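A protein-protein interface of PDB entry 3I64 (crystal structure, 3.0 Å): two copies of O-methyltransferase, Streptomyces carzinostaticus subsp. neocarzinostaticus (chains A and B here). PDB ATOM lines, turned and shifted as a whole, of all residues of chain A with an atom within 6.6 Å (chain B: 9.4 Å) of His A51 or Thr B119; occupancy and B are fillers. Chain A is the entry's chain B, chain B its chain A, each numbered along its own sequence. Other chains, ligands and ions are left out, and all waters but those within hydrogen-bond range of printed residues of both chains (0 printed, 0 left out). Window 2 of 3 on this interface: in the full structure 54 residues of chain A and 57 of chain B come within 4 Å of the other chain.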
ATOM      1  N   ALA A  41      18.626   4.355  27.431  1.00  0.00           N
ATOM      2  CA  ALA A  41      19.163   3.836  26.178  1.00  0.00           C
ATOM      3  C   ALA A  41      18.144   3.838  25.044  1.00  0.00           C
ATOM      4  O   ALA A  41      18.413   4.367  23.964  1.00  0.00           O
ATOM      5  CB  ALA A  41      19.716   2.422  26.386  1.00  0.00           C
ATOM      6  N   ALA A  45      18.854   6.375  22.030  1.00  0.00           N
ATOM      7  CA  ALA A  45      19.100   5.678  20.782  1.00  0.00           C
ATOM      8  C   ALA A  45      18.175   6.176  19.682  1.00  0.00           C
ATOM      9  O   ALA A  45      18.630   6.576  18.611  1.00  0.00           O
ATOM     10  CB  ALA A  45      18.927   4.173  20.979  1.00  0.00           C
ATOM     11  N   GLY A  49      19.410   7.954  16.711  1.00  0.00           N
ATOM     12  CA  GLY A  49      19.327   7.109  15.537  1.00  0.00           C
ATOM     13  C   GLY A  49      20.409   6.052  15.561  1.00  0.00           C
ATOM     14  O   GLY A  49      21.170   5.894  14.603  1.00  0.00           O
ATOM     15  N   ALA A  50      20.477   5.327  16.672  1.00  0.00           N
ATOM     16  CA  ALA A  50      21.462   4.271  16.856  1.00  0.00           C
ATOM     17  C   ALA A  50      20.737   2.973  17.169  1.00  0.00           C
ATOM     18  O   ALA A  50      19.524   2.964  17.352  1.00  0.00           O
ATOM     19  CB  ALA A  50      22.399   4.628  18.006  1.00  0.00           C
ATOM     20  N   HIS A  51      21.485   1.874  17.214  1.00  0.00           N
ATOM     21  CA  HIS A  51      20.909   0.578  17.543  1.00  0.00           C
ATOM     22  C   HIS A  51      20.718   0.631  19.040  1.00  0.00           C
ATOM     23  O   HIS A  51      21.690   0.712  19.789  1.00  0.00           O
ATOM     24  CB  HIS A  51      21.873  -0.552  17.209  1.00  0.00           C
ATOM     25  CG  HIS A  51      21.364  -1.901  17.601  1.00  0.00           C
ATOM     26  ND1 HIS A  51      20.401  -2.571  16.880  1.00  0.00           N
ATOM     27  CD2 HIS A  51      21.649  -2.687  18.667  1.00  0.00           C
ATOM     28  CE1 HIS A  51      20.114  -3.711  17.484  1.00  0.00           C
ATOM     29  NE2 HIS A  51      20.857  -3.804  18.571  1.00  0.00           N
ATOM     30  N   ALA A  52      19.464   0.593  19.473  1.00  0.00           N
ATOM     31  CA  ALA A  52      19.135   0.670  20.892  1.00  0.00           C
ATOM     32  C   ALA A  52      19.995  -0.189  21.825  1.00  0.00           C
ATOM     33  O   ALA A  52      20.517   0.306  22.832  1.00  0.00           O
ATOM     34  CB  ALA A  52      17.672   0.328  21.089  1.00  0.00           C
ATOM     35  N   ASP A  53      20.143  -1.468  21.494  1.00  0.00           N
ATOM     36  CA  ASP A  53      20.912  -2.371  22.337  1.00  0.00           C
ATOM     37  C   ASP A  53      22.404  -2.077  22.365  1.00  0.00           C
ATOM     38  O   ASP A  53      23.019  -2.016  23.433  1.00  0.00           O
ATOM     39  CB  ASP A  53      20.686  -3.812  21.893  1.00  0.00           C
ATOM     40  CG  ASP A  53      21.079  -4.815  22.964  1.00  0.00           C
ATOM     41  OD1 ASP A  53      22.294  -4.931  23.271  1.00  0.00           O
ATOM     42  OD2 ASP A  53      20.160  -5.479  23.510  1.00  0.00           O
ATOM     43  N   SER A  54      22.983  -1.904  21.183  1.00  0.00           N
ATOM     44  CA  SER A  54      24.407  -1.612  21.058  1.00  0.00           C
ATOM     45  C   SER A  54      24.742  -0.322  21.792  1.00  0.00           C
ATOM     46  O   SER A  54      25.718  -0.259  22.539  1.00  0.00           O
ATOM     47  CB  SER A  54      24.790  -1.470  19.581  1.00  0.00           C
ATOM     48  OG  SER A  54      24.414  -2.624  18.847  1.00  0.00           O
ATOM     49  N   LEU A  55      23.916   0.701  21.572  1.00  0.00           N
ATOM     50  CA  LEU A  55      24.116   2.003  22.193  1.00  0.00           C
ATOM     51  C   LEU A  55      24.195   1.876  23.704  1.00  0.00           C
ATOM     52  O   LEU A  55      24.976   2.584  24.345  1.00  0.00           O
ATOM     53  CB  LEU A  55      22.992   2.981  21.786  1.00  0.00           C
ATOM     54  CG  LEU A  55      23.020   4.458  22.238  1.00  0.00           C
ATOM     55  CD1 LEU A  55      22.371   4.597  23.593  1.00  0.00           C
ATOM     56  CD2 LEU A  55      24.446   4.998  22.269  1.00  0.00           C
ATOM     57  N   ASP A  56      23.410   0.969  24.283  1.00  0.00           N
ATOM     58  CA  ASP A  56      23.456   0.815  25.726  1.00  0.00           C
ATOM     59  C   ASP A  56      24.841   0.362  26.187  1.00  0.00           C
ATOM     60  O   ASP A  56      25.412   0.915  27.131  1.00  0.00           O
ATOM     61  CB  ASP A  56      22.414  -0.180  26.221  1.00  0.00           C
ATOM     62  CG  ASP A  56      22.343  -0.216  27.747  1.00  0.00           C
ATOM     63  OD1 ASP A  56      21.920   0.798  28.350  1.00  0.00           O
ATOM     64  OD2 ASP A  56      22.730  -1.243  28.351  1.00  0.00           O
ATOM     65  N   GLU B 112      35.937   1.842  13.377  1.00  0.00           N
ATOM     66  CA  GLU B 112      34.612   1.834  12.742  1.00  0.00           C
ATOM     67  C   GLU B 112      33.500   1.539  13.772  1.00  0.00           C
ATOM     68  O   GLU B 112      32.413   1.084  13.402  1.00  0.00           O
ATOM     69  CB  GLU B 112      34.557   0.776  11.643  1.00  0.00           C
ATOM     70  CG  GLU B 112      35.704   0.854  10.672  1.00  0.00           C
ATOM     71  CD  GLU B 112      35.630   2.059   9.754  1.00  0.00           C
ATOM     72  OE1 GLU B 112      36.678   2.449   9.190  1.00  0.00           O
ATOM     73  OE2 GLU B 112      34.527   2.611   9.582  1.00  0.00           O
ATOM     74  N   LEU B 113      33.776   1.794  15.054  1.00  0.00           N
ATOM     75  CA  LEU B 113      32.825   1.535  16.129  1.00  0.00           C
ATOM     76  C   LEU B 113      31.475   2.155  15.835  1.00  0.00           C
ATOM     77  O   LEU B 113      30.437   1.505  15.977  1.00  0.00           O
ATOM     78  CB  LEU B 113      33.339   2.107  17.451  1.00  0.00           C
ATOM     79  CG  LEU B 113      33.098   1.385  18.793  1.00  0.00           C
ATOM     80  CD1 LEU B 113      32.875   2.431  19.875  1.00  0.00           C
ATOM     81  CD2 LEU B 113      31.934   0.426  18.720  1.00  0.00           C
ATOM     82  N   ALA B 114      31.494   3.424  15.432  1.00  0.00           N
ATOM     83  CA  ALA B 114      30.271   4.164  15.134  1.00  0.00           C
ATOM     84  C   ALA B 114      29.276   3.323  14.336  1.00  0.00           C
ATOM     85  O   ALA B 114      28.072   3.374  14.578  1.00  0.00           O
ATOM     86  CB  ALA B 114      30.608   5.440  14.392  1.00  0.00           C
ATOM     87  N   HIS B 115      29.778   2.526  13.402  1.00  0.00           N
ATOM     88  CA  HIS B 115      28.903   1.690  12.599  1.00  0.00           C
ATOM     89  C   HIS B 115      28.208   0.628  13.431  1.00  0.00           C
ATOM     90  O   HIS B 115      27.026   0.356  13.247  1.00  0.00           O
ATOM     91  CB  HIS B 115      29.679   0.996  11.489  1.00  0.00           C
ATOM     92  CG  HIS B 115      28.884  -0.057  10.791  1.00  0.00           C
ATOM     93  ND1 HIS B 115      27.750   0.232  10.065  1.00  0.00           N
ATOM     94  CD2 HIS B 115      29.007  -1.405  10.779  1.00  0.00           C
ATOM     95  CE1 HIS B 115      27.207  -0.893   9.638  1.00  0.00           C
ATOM     96  NE2 HIS B 115      27.949  -1.902  10.058  1.00  0.00           N
ATOM     97  N   SER B 116      28.952   0.014  14.339  1.00  0.00           N
ATOM     98  CA  SER B 116      28.390  -1.028  15.179  1.00  0.00           C
ATOM     99  C   SER B 116      27.338  -0.518  16.129  1.00  0.00           C
ATOM    100  O   SER B 116      26.248  -1.078  16.199  1.00  0.00           O
ATOM    101  CB  SER B 116      29.478  -1.730  15.999  1.00  0.00           C
ATOM    102  OG  SER B 116      30.073  -2.773  15.260  1.00  0.00           O
ATOM    103  N   ILE B 117      27.658   0.541  16.871  1.00  0.00           N
ATOM    104  CA  ILE B 117      26.698   1.036  17.846  1.00  0.00           C
ATOM    105  C   ILE B 117      25.541   1.717  17.125  1.00  0.00           C
ATOM    106  O   ILE B 117      24.505   2.015  17.714  1.00  0.00           O
ATOM    107  CB  ILE B 117      27.379   1.975  18.905  1.00  0.00           C
ATOM    108  CG1 ILE B 117      27.051   3.432  18.630  1.00  0.00           C
ATOM    109  CG2 ILE B 117      28.867   1.771  18.909  1.00  0.00           C
ATOM    110  CD1 ILE B 117      25.812   3.897  19.348  1.00  0.00           C
ATOM    111  N   ARG B 118      25.711   1.915  15.830  1.00  0.00           N
ATOM    112  CA  ARG B 118      24.683   2.547  15.029  1.00  0.00           C
ATOM    113  C   ARG B 118      23.723   1.509  14.456  1.00  0.00           C
ATOM    114  O   ARG B 118      22.537   1.765  14.329  1.00  0.00           O
ATOM    115  CB  ARG B 118      25.342   3.320  13.886  1.00  0.00           C
ATOM    116  CG  ARG B 118      24.441   4.296  13.164  1.00  0.00           C
ATOM    117  CD  ARG B 118      25.099   4.818  11.873  1.00  0.00           C
ATOM    118  NE  ARG B 118      26.178   5.796  12.065  1.00  0.00           N
ATOM    119  CZ  ARG B 118      26.046   6.958  12.707  1.00  0.00           C
ATOM    120  NH1 ARG B 118      24.876   7.297  13.246  1.00  0.00           N
ATOM    121  NH2 ARG B 118      27.071   7.807  12.772  1.00  0.00           N
ATOM    122  N   THR B 119      24.233   0.325  14.138  1.00  0.00           N
ATOM    123  CA  THR B 119      23.422  -0.722  13.522  1.00  0.00           C
ATOM    124  C   THR B 119      23.325  -2.035  14.281  1.00  0.00           C
ATOM    125  O   THR B 119      22.450  -2.852  13.993  1.00  0.00           O
ATOM    126  CB  THR B 119      23.972  -1.076  12.146  1.00  0.00           C
ATOM    127  OG1 THR B 119      25.091  -1.960  12.299  1.00  0.00           O
ATOM    128  CG2 THR B 119      24.437   0.180  11.426  1.00  0.00           C
ATOM    129  N   GLY B 120      24.228  -2.255  15.228  1.00  0.00           N
ATOM    130  CA  GLY B 120      24.215  -3.495  15.976  1.00  0.00           C
ATOM    131  C   GLY B 120      25.014  -4.563  15.252  1.00  0.00           C
ATOM    132  O   GLY B 120      25.172  -5.669  15.746  1.00  0.00           O
ATOM    133  N   GLN B 121      25.519  -4.245  14.068  1.00  0.00           N
ATOM    134  CA  GLN B 121      26.312  -5.204  13.310  1.00  0.00           C
ATOM    135  C   GLN B 121      27.806  -5.126  13.661  1.00  0.00           C
ATOM    136  O   GLN B 121      28.247  -4.183  14.314  1.00  0.00           O
ATOM    137  CB  GLN B 121      26.102  -4.964  11.809  1.00  0.00           C
ATOM    138  CG  GLN B 121      24.765  -5.489  11.284  1.00  0.00           C
ATOM    139  CD  GLN B 121      24.582  -7.003  11.517  1.00  0.00           C
ATOM    140  OE1 GLN B 121      24.418  -7.465  12.657  1.00  0.00           O
ATOM    141  NE2 GLN B 121      24.615  -7.776  10.431  1.00  0.00           N
ATOM    142  N   PRO B 122      28.603  -6.128  13.260  1.00  0.00           N
ATOM    143  CA  PRO B 122      30.029  -6.057  13.586  1.00  0.00           C
ATOM    144  C   PRO B 122      30.714  -4.977  12.762  1.00  0.00           C
ATOM    145  O   PRO B 122      30.227  -4.595  11.694  1.00  0.00           O
ATOM    146  CB  PRO B 122      30.523  -7.458  13.260  1.00  0.00           C
ATOM    147  CG  PRO B 122      29.658  -7.856  12.167  1.00  0.00           C
ATOM    148  CD  PRO B 122      28.294  -7.420  12.639  1.00  0.00           C
ATOM    149  N   ALA B 123      31.844  -4.489  13.261  1.00  0.00           N
ATOM    150  CA  ALA B 123      32.575  -3.427  12.598  1.00  0.00           C
ATOM    151  C   ALA B 123      33.796  -3.923  11.840  1.00  0.00           C
ATOM    152  O   ALA B 123      34.251  -3.279  10.887  1.00  0.00           O
ATOM    153  CB  ALA B 123      32.987  -2.389  13.626  1.00  0.00           C
ATOM    154  N   VAL B 126      33.441  -3.872   8.138  1.00  0.00           N
ATOM    155  CA  VAL B 126      33.495  -2.529   7.577  1.00  0.00           C
ATOM    156  C   VAL B 126      34.907  -2.137   7.203  1.00  0.00           C
ATOM    157  O   VAL B 126      35.129  -1.582   6.133  1.00  0.00           O
ATOM    158  CB  VAL B 126      32.956  -1.457   8.551  1.00  0.00           C
ATOM    159  CG1 VAL B 126      33.080  -0.084   7.923  1.00  0.00           C
ATOM    160  CG2 VAL B 126      31.515  -1.735   8.895  1.00  0.00           C
ATOM    161  N   ASP B 250      23.256 -13.776  19.881  1.00  0.00           N
ATOM    162  CA  ASP B 250      22.328 -14.703  20.520  1.00  0.00           C
ATOM    163  C   ASP B 250      21.826 -15.862  19.681  1.00  0.00           C
ATOM    164  O   ASP B 250      21.835 -17.010  20.136  1.00  0.00           O
ATOM    165  CB  ASP B 250      21.125 -13.954  21.081  1.00  0.00           C
ATOM    166  CG  ASP B 250      21.461 -13.167  22.317  1.00  0.00           C
ATOM    167  OD1 ASP B 250      22.060 -13.756  23.240  1.00  0.00           O
ATOM    168  OD2 ASP B 250      21.123 -11.969  22.372  1.00  0.00           O
ATOM    169  N   LEU B 291      31.508  -6.912  20.287  1.00  0.00           N
ATOM    170  CA  LEU B 291      30.540  -6.296  19.383  1.00  0.00           C
ATOM    171  C   LEU B 291      31.268  -5.856  18.124  1.00  0.00           C
ATOM    172  O   LEU B 291      30.829  -6.132  17.004  1.00  0.00           O
ATOM    173  CB  LEU B 291      29.899  -5.079  20.055  1.00  0.00           C
ATOM    174  CG  LEU B 291      29.082  -4.039  19.274  1.00  0.00           C
ATOM    175  CD1 LEU B 291      27.844  -4.650  18.620  1.00  0.00           C
ATOM    176  CD2 LEU B 291      28.701  -2.951  20.251  1.00  0.00           C
ATOM    177  N   GLY B 295      29.784  -8.831  16.622  1.00  0.00           N
ATOM    178  CA  GLY B 295      28.426  -8.598  17.068  1.00  0.00           C
ATOM    179  C   GLY B 295      28.194  -9.621  18.169  1.00  0.00           C
ATOM    180  O   GLY B 295      27.080 -10.098  18.400  1.00  0.00           O
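Among the printed residues, merely in contact across the chains: Ser A54 with Gly B120, Ala A50 with Ile B117, Leu A55 with Ile B117, His A51 with Gly B120, His A51 with Thr B119, Ala A50 with Arg B118, Ser A54 with Ser B116, Ser A54 with Ile B117, Gly A49 with Arg B118 and Ser A54 with Leu B291.
The backbone carbonyl oxygen of His B115 sits at hydrogen-bond distance from the side-chain hydroxyl of Thr B119, 3.2 Å away. The backbone carbonyl oxygen (O) of Ala A45 sits at hydrogen-bond distance from the backbone NH (N) of Ala A50 (3.0 Å). The backbone NH (N) of Gln B121 is in hydrogen-bond range of the side-chain hydroxyl (OG1) of Thr B119. The backbone carbonyl oxygen (O) of Gln B121 sits at hydrogen-bond distance from the side-chain hydroxyl (OG) of Ser B116, at 2.5 Å. OG of Ser B116 sits at hydrogen-bond distance from N of Ala B123 (3.2 Å).
Of the 10 printed residues of chain A, 5 touch a printed residue of chain B. Hydrophobic or aromatic side chains of chain A that line the printed part of chain B: Ala A50, His A51 and Leu A55. Printed residues of chain B that touch a printed residue of chain A: Ser B116, Ile B117, Arg B118, Thr B119, Gly B120 and Leu B291.
No position is printed for both chains.
His A51 touches just these residues of chain B: Ile B117 (3.1 Å), Arg B118 (3.1 Å), Thr B119 (3.6 Å) and Gly B120 (3.5 Å). Of chain A, only His A51 comes within 4 Å of Thr B119. Of chain B, only Ile B117 (3.4 Å) and Arg B118 (3.6 Å) come within 4 Å of Ala A50. No residue of chain B comes within 4 Å of Ala A52. No residue of chain B comes within 4 Å of Asp A53. Printed residues of chain B within 4 Å of Gly A49: Arg B118. Printed residues of chain A within 4 Å of Arg B118: Gly A49, Ala A50 and His A51. Of the printed residues of chain A, Ile B117 touches Ala A50, His A51, Ser A54 and Leu A55. Of the printed residues of chain B, Leu A55 touches Ile B117. Gln B121 touches none of the printed residues of chain A. The nearest residue of chain B that does not touch His A51 is Ser B116 (4.5 Å). The nearest printed residue of chain A that does not touch Arg B118 is Ser A54 (5.1 Å).
The backbone carbonyl oxygen (O) of Arg B118 sits at hydrogen-bond distance from the backbone NH (N) of His A51 (3.1 Å). The backbone NH of His A51 sits at hydrogen-bond distance from the backbone carbonyl oxygen of Ile B117 (3.1 Å).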
